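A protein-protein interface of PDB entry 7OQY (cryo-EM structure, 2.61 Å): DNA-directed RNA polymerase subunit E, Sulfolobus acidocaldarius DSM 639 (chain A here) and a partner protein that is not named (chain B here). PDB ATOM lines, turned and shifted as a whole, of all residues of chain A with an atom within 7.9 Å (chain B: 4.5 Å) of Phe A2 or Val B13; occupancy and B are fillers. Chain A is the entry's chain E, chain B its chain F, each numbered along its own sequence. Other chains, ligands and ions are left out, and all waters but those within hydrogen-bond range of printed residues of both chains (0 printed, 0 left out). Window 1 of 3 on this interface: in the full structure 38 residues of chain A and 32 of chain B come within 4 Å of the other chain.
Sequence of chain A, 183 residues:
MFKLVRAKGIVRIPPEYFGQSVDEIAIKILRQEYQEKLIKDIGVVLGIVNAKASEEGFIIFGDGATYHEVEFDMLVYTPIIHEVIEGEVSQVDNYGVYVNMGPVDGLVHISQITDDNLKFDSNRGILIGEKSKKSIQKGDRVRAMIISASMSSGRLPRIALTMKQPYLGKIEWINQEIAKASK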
ATOM      1  N   MET A   1      11.287  15.359  10.682  1.00  0.00           N
ATOM      2  CA  MET A   1      10.868  13.962  10.660  1.00  0.00           C
ATOM      3  C   MET A   1      12.073  13.031  10.740  1.00  0.00           C
ATOM      4  O   MET A   1      13.095  13.266  10.095  1.00  0.00           O
ATOM      5  CB  MET A   1      10.056  13.666   9.398  1.00  0.00           C
ATOM      6  N   PHE A   2      11.945  11.971  11.534  1.00  0.00           N
ATOM      7  CA  PHE A   2      13.017  11.001  11.717  1.00  0.00           C
ATOM      8  C   PHE A   2      13.085  10.095  10.492  1.00  0.00           C
ATOM      9  O   PHE A   2      12.053   9.623  10.004  1.00  0.00           O
ATOM     10  CB  PHE A   2      12.799  10.177  12.985  1.00  0.00           C
ATOM     11  CG  PHE A   2      13.262  10.861  14.241  1.00  0.00           C
ATOM     12  CD1 PHE A   2      12.805  12.127  14.567  1.00  0.00           C
ATOM     13  CD2 PHE A   2      14.163  10.240  15.090  1.00  0.00           C
ATOM     14  CE1 PHE A   2      13.231  12.758  15.720  1.00  0.00           C
ATOM     15  CE2 PHE A   2      14.594  10.867  16.244  1.00  0.00           C
ATOM     16  CZ  PHE A   2      14.128  12.128  16.559  1.00  0.00           C
ATOM     17  N   LYS A   3      14.296   9.859  10.000  1.00  0.00           N
ATOM     18  CA  LYS A   3      14.528   9.042   8.819  1.00  0.00           C
ATOM     19  C   LYS A   3      15.556   7.956   9.121  1.00  0.00           C
ATOM     20  O   LYS A   3      16.259   7.988  10.135  1.00  0.00           O
ATOM     21  CB  LYS A   3      14.985   9.914   7.646  1.00  0.00           C
ATOM     22  CG  LYS A   3      13.856  10.630   6.924  1.00  0.00           C
ATOM     23  CD  LYS A   3      14.317  11.186   5.586  1.00  0.00           C
ATOM     24  CE  LYS A   3      15.631  11.940   5.717  1.00  0.00           C
ATOM     25  NZ  LYS A   3      15.536  13.063   6.691  1.00  0.00           N
ATOM     26  N   LEU A   4      15.633   6.977   8.219  1.00  0.00           N
ATOM     27  CA  LEU A   4      16.651   5.930   8.290  1.00  0.00           C
ATOM     28  C   LEU A   4      17.090   5.648   6.857  1.00  0.00           C
ATOM     29  O   LEU A   4      16.332   5.066   6.076  1.00  0.00           O
ATOM     30  CB  LEU A   4      16.119   4.680   8.981  1.00  0.00           C
ATOM     31  CG  LEU A   4      17.112   3.554   9.295  1.00  0.00           C
ATOM     32  CD1 LEU A   4      16.647   2.768  10.502  1.00  0.00           C
ATOM     33  CD2 LEU A   4      17.304   2.612   8.112  1.00  0.00           C
ATOM     34  N   VAL A   5      18.306   6.064   6.523  1.00  0.00           N
ATOM     35  CA  VAL A   5      18.828   5.920   5.177  1.00  0.00           C
ATOM     36  C   VAL A   5      19.914   4.853   5.170  1.00  0.00           C
ATOM     37  O   VAL A   5      20.559   4.567   6.183  1.00  0.00           O
ATOM     38  CB  VAL A   5      19.367   7.260   4.625  1.00  0.00           C
ATOM     39  CG1 VAL A   5      18.306   8.338   4.732  1.00  0.00           C
ATOM     40  CG2 VAL A   5      20.630   7.673   5.363  1.00  0.00           C
ATOM     41  N   LEU A  46      22.532  11.027  13.547  1.00  0.00           N
ATOM     42  CA  LEU A  46      22.351  10.634  14.938  1.00  0.00           C
ATOM     43  C   LEU A  46      23.027   9.309  15.273  1.00  0.00           C
ATOM     44  O   LEU A  46      22.782   8.756  16.351  1.00  0.00           O
ATOM     45  CB  LEU A  46      20.861  10.562  15.281  1.00  0.00           C
ATOM     46  CG  LEU A  46      20.170  11.859  15.714  1.00  0.00           C
ATOM     47  CD1 LEU A  46      19.966  12.804  14.538  1.00  0.00           C
ATOM     48  CD2 LEU A  46      18.846  11.557  16.398  1.00  0.00           C
ATOM     49  N   MET A  74      21.898   4.501   8.544  1.00  0.00           N
ATOM     50  CA  MET A  74      22.025   5.683   9.377  1.00  0.00           C
ATOM     51  C   MET A  74      20.711   5.951  10.107  1.00  0.00           C
ATOM     52  O   MET A  74      19.693   5.298   9.871  1.00  0.00           O
ATOM     53  CB  MET A  74      22.443   6.882   8.524  1.00  0.00           C
ATOM     54  CG  MET A  74      23.841   6.755   7.944  1.00  0.00           C
ATOM     55  SD  MET A  74      24.166   7.934   6.620  1.00  0.00           S
ATOM     56  CE  MET A  74      24.813   9.315   7.551  1.00  0.00           C
ATOM     57  N   LEU A  75      20.737   6.928  11.009  1.00  0.00           N
ATOM     58  CA  LEU A  75      19.556   7.358  11.753  1.00  0.00           C
ATOM     59  C   LEU A  75      19.431   8.877  11.676  1.00  0.00           C
ATOM     60  O   LEU A  75      19.250   9.578  12.673  1.00  0.00           O
ATOM     61  CB  LEU A  75      19.612   6.855  13.196  1.00  0.00           C
ATOM     62  CG  LEU A  75      18.382   7.057  14.090  1.00  0.00           C
ATOM     63  CD1 LEU A  75      17.179   6.322  13.521  1.00  0.00           C
ATOM     64  CD2 LEU A  75      18.666   6.604  15.513  1.00  0.00           C
ATOM     65  N   VAL A  76      19.559   9.404  10.458  1.00  0.00           N
ATOM     66  CA  VAL A  76      19.498  10.842  10.245  1.00  0.00           C
ATOM     67  C   VAL A  76      18.093  11.362  10.534  1.00  0.00           C
ATOM     68  O   VAL A  76      17.083  10.697  10.261  1.00  0.00           O
ATOM     69  CB  VAL A  76      19.945  11.189   8.812  1.00  0.00           C
ATOM     70  CG1 VAL A  76      18.946  10.660   7.791  1.00  0.00           C
ATOM     71  CG2 VAL A  76      20.123  12.687   8.656  1.00  0.00           C
ATOM     72  N   TYR A  77      18.028  12.556  11.117  1.00  0.00           N
ATOM     73  CA  TYR A  77      16.775  13.251  11.372  1.00  0.00           C
ATOM     74  C   TYR A  77      16.836  14.643  10.764  1.00  0.00           C
ATOM     75  O   TYR A  77      17.808  15.378  10.966  1.00  0.00           O
ATOM     76  CB  TYR A  77      16.484  13.348  12.874  1.00  0.00           C
ATOM     77  CG  TYR A  77      15.709  14.587  13.269  1.00  0.00           C
ATOM     78  CD1 TYR A  77      14.350  14.695  13.004  1.00  0.00           C
ATOM     79  CD2 TYR A  77      16.337  15.647  13.909  1.00  0.00           C
ATOM     80  CE1 TYR A  77      13.640  15.826  13.362  1.00  0.00           C
ATOM     81  CE2 TYR A  77      15.635  16.781  14.272  1.00  0.00           C
ATOM     82  CZ  TYR A  77      14.288  16.865  13.997  1.00  0.00           C
ATOM     83  OH  TYR A  77      13.586  17.992  14.356  1.00  0.00           O
ATOM     84  N   THR A  78      15.790  15.003  10.018  1.00  0.00           N
ATOM     85  CA  THR A  78      15.697  16.316   9.403  1.00  0.00           C
ATOM     86  C   THR A  78      14.249  16.780   9.514  1.00  0.00           C
ATOM     87  O   THR A  78      13.334  16.057   9.081  1.00  0.00           O
ATOM     88  CB  THR A  78      16.142  16.292   7.937  1.00  0.00           C
ATOM     89  OG1 THR A  78      17.478  15.782   7.849  1.00  0.00           O
ATOM     90  CG2 THR A  78      16.106  17.694   7.345  1.00  0.00           C
ATOM     91  N   PRO A  79      14.003  17.964  10.080  1.00  0.00           N
ATOM     92  CA  PRO A  79      12.628  18.483  10.156  1.00  0.00           C
ATOM     93  C   PRO A  79      12.175  18.990   8.795  1.00  0.00           C
ATOM     94  O   PRO A  79      12.792  19.885   8.213  1.00  0.00           O
ATOM     95  CB  PRO A  79      12.731  19.619  11.181  1.00  0.00           C
ATOM     96  CG  PRO A  79      14.164  20.023  11.192  1.00  0.00           C
ATOM     97  CD  PRO A  79      14.997  18.910  10.615  1.00  0.00           C
ATOM     98  N   ILE A  80      11.090  18.413   8.289  1.00  0.00           N
ATOM     99  CA  ILE A  80      10.574  18.734   6.963  1.00  0.00           C
ATOM    100  C   ILE A  80       9.569  19.871   7.087  1.00  0.00           C
ATOM    101  O   ILE A  80       8.765  19.903   8.026  1.00  0.00           O
ATOM    102  CB  ILE A  80       9.938  17.495   6.309  1.00  0.00           C
ATOM    103  CG1 ILE A  80      11.003  16.424   6.058  1.00  0.00           C
ATOM    104  CG2 ILE A  80       9.233  17.863   5.008  1.00  0.00           C
ATOM    105  CD1 ILE A  80      11.937  16.746   4.911  1.00  0.00           C
ATOM    106  N   GLU A  83       5.003  20.330   8.502  1.00  0.00           N
ATOM    107  CA  GLU A  83       4.718  19.101   9.227  1.00  0.00           C
ATOM    108  C   GLU A  83       4.270  19.446  10.639  1.00  0.00           C
ATOM    109  O   GLU A  83       4.730  20.432  11.223  1.00  0.00           O
ATOM    110  CB  GLU A  83       5.939  18.166   9.250  1.00  0.00           C
ATOM    111  CG  GLU A  83       6.950  18.447  10.350  1.00  0.00           C
ATOM    112  CD  GLU A  83       7.956  17.324  10.513  1.00  0.00           C
ATOM    113  OE1 GLU A  83       7.781  16.268   9.869  1.00  0.00           O
ATOM    114  OE2 GLU A  83       8.923  17.497  11.284  1.00  0.00           O
ATOM    115  N   ILE A  85       4.275  18.461  14.422  1.00  0.00           N
ATOM    116  CA  ILE A  85       5.086  17.684  15.351  1.00  0.00           C
ATOM    117  C   ILE A  85       4.853  18.198  16.763  1.00  0.00           C
ATOM    118  O   ILE A  85       4.756  19.409  16.990  1.00  0.00           O
ATOM    119  CB  ILE A  85       6.584  17.743  14.987  1.00  0.00           C
ATOM    120  CG1 ILE A  85       7.012  19.185  14.702  1.00  0.00           C
ATOM    121  CG2 ILE A  85       6.882  16.839  13.801  1.00  0.00           C
ATOM    122  CD1 ILE A  85       8.481  19.331  14.369  1.00  0.00           C
ATOM    123  N   MET A 101      12.823  19.980  20.120  1.00  0.00           N
ATOM    124  CA  MET A 101      12.491  19.054  19.035  1.00  0.00           C
ATOM    125  C   MET A 101      13.621  18.033  18.937  1.00  0.00           C
ATOM    126  O   MET A 101      14.532  18.185  18.120  1.00  0.00           O
ATOM    127  CB  MET A 101      12.290  19.793  17.716  1.00  0.00           C
ATOM    128  CG  MET A 101      11.103  20.737  17.692  1.00  0.00           C
ATOM    129  SD  MET A 101       9.535  19.872  17.885  1.00  0.00           S
ATOM    130  CE  MET A 101       8.410  21.254  18.048  1.00  0.00           C
ATOM    131  N   GLY A 102      13.548  16.987  19.756  1.00  0.00           N
ATOM    132  CA  GLY A 102      14.577  15.977  19.792  1.00  0.00           C
ATOM    133  C   GLY A 102      15.936  16.547  20.141  1.00  0.00           C
ATOM    134  O   GLY A 102      16.112  17.217  21.163  1.00  0.00           O
ATOM    135  N   PRO A 103      16.934  16.275  19.297  1.00  0.00           N
ATOM    136  CA  PRO A 103      18.279  16.816  19.555  1.00  0.00           C
ATOM    137  C   PRO A 103      18.341  18.334  19.567  1.00  0.00           C
ATOM    138  O   PRO A 103      19.132  18.903  20.331  1.00  0.00           O
ATOM    139  CB  PRO A 103      19.117  16.223  18.412  1.00  0.00           C
ATOM    140  CG  PRO A 103      18.125  15.899  17.340  1.00  0.00           C
ATOM    141  CD  PRO A 103      16.887  15.468  18.065  1.00  0.00           C
ATOM    142  N   HIS B  11      13.845   5.812   3.344  1.00  0.00           N
ATOM    143  CA  HIS B  11      12.705   5.399   4.150  1.00  0.00           C
ATOM    144  C   HIS B  11      12.428   6.406   5.263  1.00  0.00           C
ATOM    145  O   HIS B  11      13.316   7.141   5.703  1.00  0.00           O
ATOM    146  CB  HIS B  11      12.948   4.013   4.745  1.00  0.00           C
ATOM    147  CG  HIS B  11      12.635   2.889   3.807  1.00  0.00           C
ATOM    148  ND1 HIS B  11      11.481   2.846   3.055  1.00  0.00           N
ATOM    149  CD2 HIS B  11      13.326   1.766   3.500  1.00  0.00           C
ATOM    150  CE1 HIS B  11      11.475   1.745   2.324  1.00  0.00           C
ATOM    151  NE2 HIS B  11      12.583   1.072   2.576  1.00  0.00           N
ATOM    152  N   PHE B  12      11.177   6.431   5.714  1.00  0.00           N
ATOM    153  CA  PHE B  12      10.730   7.335   6.763  1.00  0.00           C
ATOM    154  C   PHE B  12      10.447   6.555   8.041  1.00  0.00           C
ATOM    155  O   PHE B  12      10.053   5.386   8.003  1.00  0.00           O
ATOM    156  CB  PHE B  12       9.479   8.105   6.332  1.00  0.00           C
ATOM    157  CG  PHE B  12       9.778   9.426   5.682  1.00  0.00           C
ATOM    158  CD1 PHE B  12       9.994  10.558   6.448  1.00  0.00           C
ATOM    159  CD2 PHE B  12       9.855   9.531   4.303  1.00  0.00           C
ATOM    160  CE1 PHE B  12      10.272  11.773   5.853  1.00  0.00           C
ATOM    161  CE2 PHE B  12      10.132  10.743   3.700  1.00  0.00           C
ATOM    162  CZ  PHE B  12      10.343  11.866   4.477  1.00  0.00           C
ATOM    163  N   VAL B  13      10.652   7.216   9.177  1.00  0.00           N
ATOM    164  CA  VAL B  13      10.568   6.562  10.481  1.00  0.00           C
ATOM    165  C   VAL B  13       9.701   7.387  11.427  1.00  0.00           C
ATOM    166  O   VAL B  13      10.011   8.558  11.688  1.00  0.00           O
ATOM    167  CB  VAL B  13      11.969   6.339  11.073  1.00  0.00           C
ATOM    168  CG1 VAL B  13      11.878   5.950  12.536  1.00  0.00           C
ATOM    169  CG2 VAL B  13      12.716   5.275  10.282  1.00  0.00           C
ATOM    170  N   PRO B  14       8.619   6.829  11.958  1.00  0.00           N
ATOM    171  CA  PRO B  14       7.807   7.539  12.951  1.00  0.00           C
ATOM    172  C   PRO B  14       8.514   7.578  14.303  1.00  0.00           C
ATOM    173  O   PRO B  14       9.637   7.107  14.462  1.00  0.00           O
ATOM    174  CB  PRO B  14       6.521   6.711  13.010  1.00  0.00           C
ATOM    175  CG  PRO B  14       6.936   5.344  12.594  1.00  0.00           C
ATOM    176  CD  PRO B  14       8.026   5.535  11.579  1.00  0.00           C
ATOM    177  N   TYR B  15       7.823   8.153  15.291  1.00  0.00           N
ATOM    178  CA  TYR B  15       8.432   8.348  16.605  1.00  0.00           C
ATOM    179  C   TYR B  15       8.635   7.027  17.338  1.00  0.00           C
ATOM    180  O   TYR B  15       9.630   6.857  18.052  1.00  0.00           O
ATOM    181  CB  TYR B  15       7.575   9.293  17.447  1.00  0.00           C
ATOM    182  CG  TYR B  15       7.834  10.761  17.194  1.00  0.00           C
ATOM    183  CD1 TYR B  15       8.543  11.182  16.077  1.00  0.00           C
ATOM    184  CD2 TYR B  15       7.371  11.727  18.079  1.00  0.00           C
ATOM    185  CE1 TYR B  15       8.781  12.524  15.846  1.00  0.00           C
ATOM    186  CE2 TYR B  15       7.605  13.070  17.857  1.00  0.00           C
ATOM    187  CZ  TYR B  15       8.310  13.463  16.739  1.00  0.00           C
ATOM    188  OH  TYR B  15       8.545  14.800  16.513  1.00  0.00           O
ATOM    189  N   ILE B  17       9.119   3.686  16.389  1.00  0.00           N
ATOM    190  CA  ILE B  17      10.231   2.809  16.036  1.00  0.00           C
ATOM    191  C   ILE B  17      11.545   3.578  16.060  1.00  0.00           C
ATOM    192  O   ILE B  17      12.624   2.974  16.101  1.00  0.00           O
ATOM    193  CB  ILE B  17       9.993   2.130  14.674  1.00  0.00           C
ATOM    194  CG1 ILE B  17       9.884   3.166  13.558  1.00  0.00           C
ATOM    195  CG2 ILE B  17       8.745   1.261  14.721  1.00  0.00           C
ATOM    196  CD1 ILE B  17       9.952   2.561  12.172  1.00  0.00           C
ATOM    197  N   ALA B  18      11.485   4.911  16.028  1.00  0.00           N
ATOM    198  CA  ALA B  18      12.682   5.703  16.285  1.00  0.00           C
ATOM    199  C   ALA B  18      13.181   5.477  17.706  1.00  0.00           C
ATOM    200  O   ALA B  18      14.392   5.427  17.947  1.00  0.00           O
ATOM    201  CB  ALA B  18      12.402   7.186  16.042  1.00  0.00           C
ATOM    202  N   THR B  38      18.060  12.797  23.124  1.00  0.00           N
ATOM    203  CA  THR B  38      16.973  12.542  22.183  1.00  0.00           C
ATOM    204  C   THR B  38      16.096  11.388  22.658  1.00  0.00           C
ATOM    205  O   THR B  38      14.876  11.398  22.452  1.00  0.00           O
ATOM    206  CB  THR B  38      17.544  12.254  20.793  1.00  0.00           C
ATOM    207  OG1 THR B  38      18.262  13.404  20.325  1.00  0.00           O
ATOM    208  CG2 THR B  38      16.432  11.931  19.805  1.00  0.00           C
ATOM    209  N   ALA B  71       4.343   8.502   8.335  1.00  0.00           N
ATOM    210  CA  ALA B  71       5.242   8.505   9.480  1.00  0.00           C
ATOM    211  C   ALA B  71       4.873   9.553  10.523  1.00  0.00           C
ATOM    212  O   ALA B  71       5.343   9.464  11.662  1.00  0.00           O
ATOM    213  CB  ALA B  71       6.684   8.731   9.019  1.00  0.00           C
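The backbone NH (N) of Lys A3 lies within hydrogen-bond range of the backbone carbonyl oxygen (O) of Val A76 (2.9 Å).
Among the printed residues, pairs that only touch across the chains: Phe A2 with Ala B18 (3.7 Å), Leu A4 with Val B13 (3.7 Å), Lys A3 with His B11 (3.7 Å), Ile A85 with Tyr B15 (3.8 Å), Lys A3 with Phe B12 (3.9 Å), Gly A102 with Thr B38 (3.9 Å), Phe A2 with Phe B12 (3.98 Å) and Phe A2 with Thr B38 (3.99 Å).
O of Phe A2 is in hydrogen-bond range of N of Val B13, at 2.9 Å. N of Leu A4 sits at hydrogen-bond distance from O of His B11 (3.4 Å). The backbone nitrogen of Pro A103 lies close to the side-chain hydroxyl of Thr B38.
Of the 18 printed residues of chain A, 6 touch a printed residue of chain B. Printed residues of chain A that touch a printed residue of chain B: Phe A2, Lys A3, Leu A4, Ile A85, Gly A102 and Pro A103. Among the printed residues, no Asp or Glu carboxylate lies within 4 Å of a Lys or Arg side-chain nitrogen of the other chain.
Met A1 touches none of the printed residues of chain B. Printed residues of chain B within 4 Å of Phe A2: Phe B12, Val B13, Ala B18 and Thr B38. Leu A75 touches none of the printed residues of chain B. Of the printed residues of chain A, His B11 touches Lys A3 (3.7 Å) and Leu A4 (3.4 Å). No residue of chain A comes within 4 Å of Pro B14. Of the printed residues of chain A, Tyr B15 touches Ile A85. The nearest residue of chain A that does not touch Val B13 is Lys A3 (4.1 Å).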
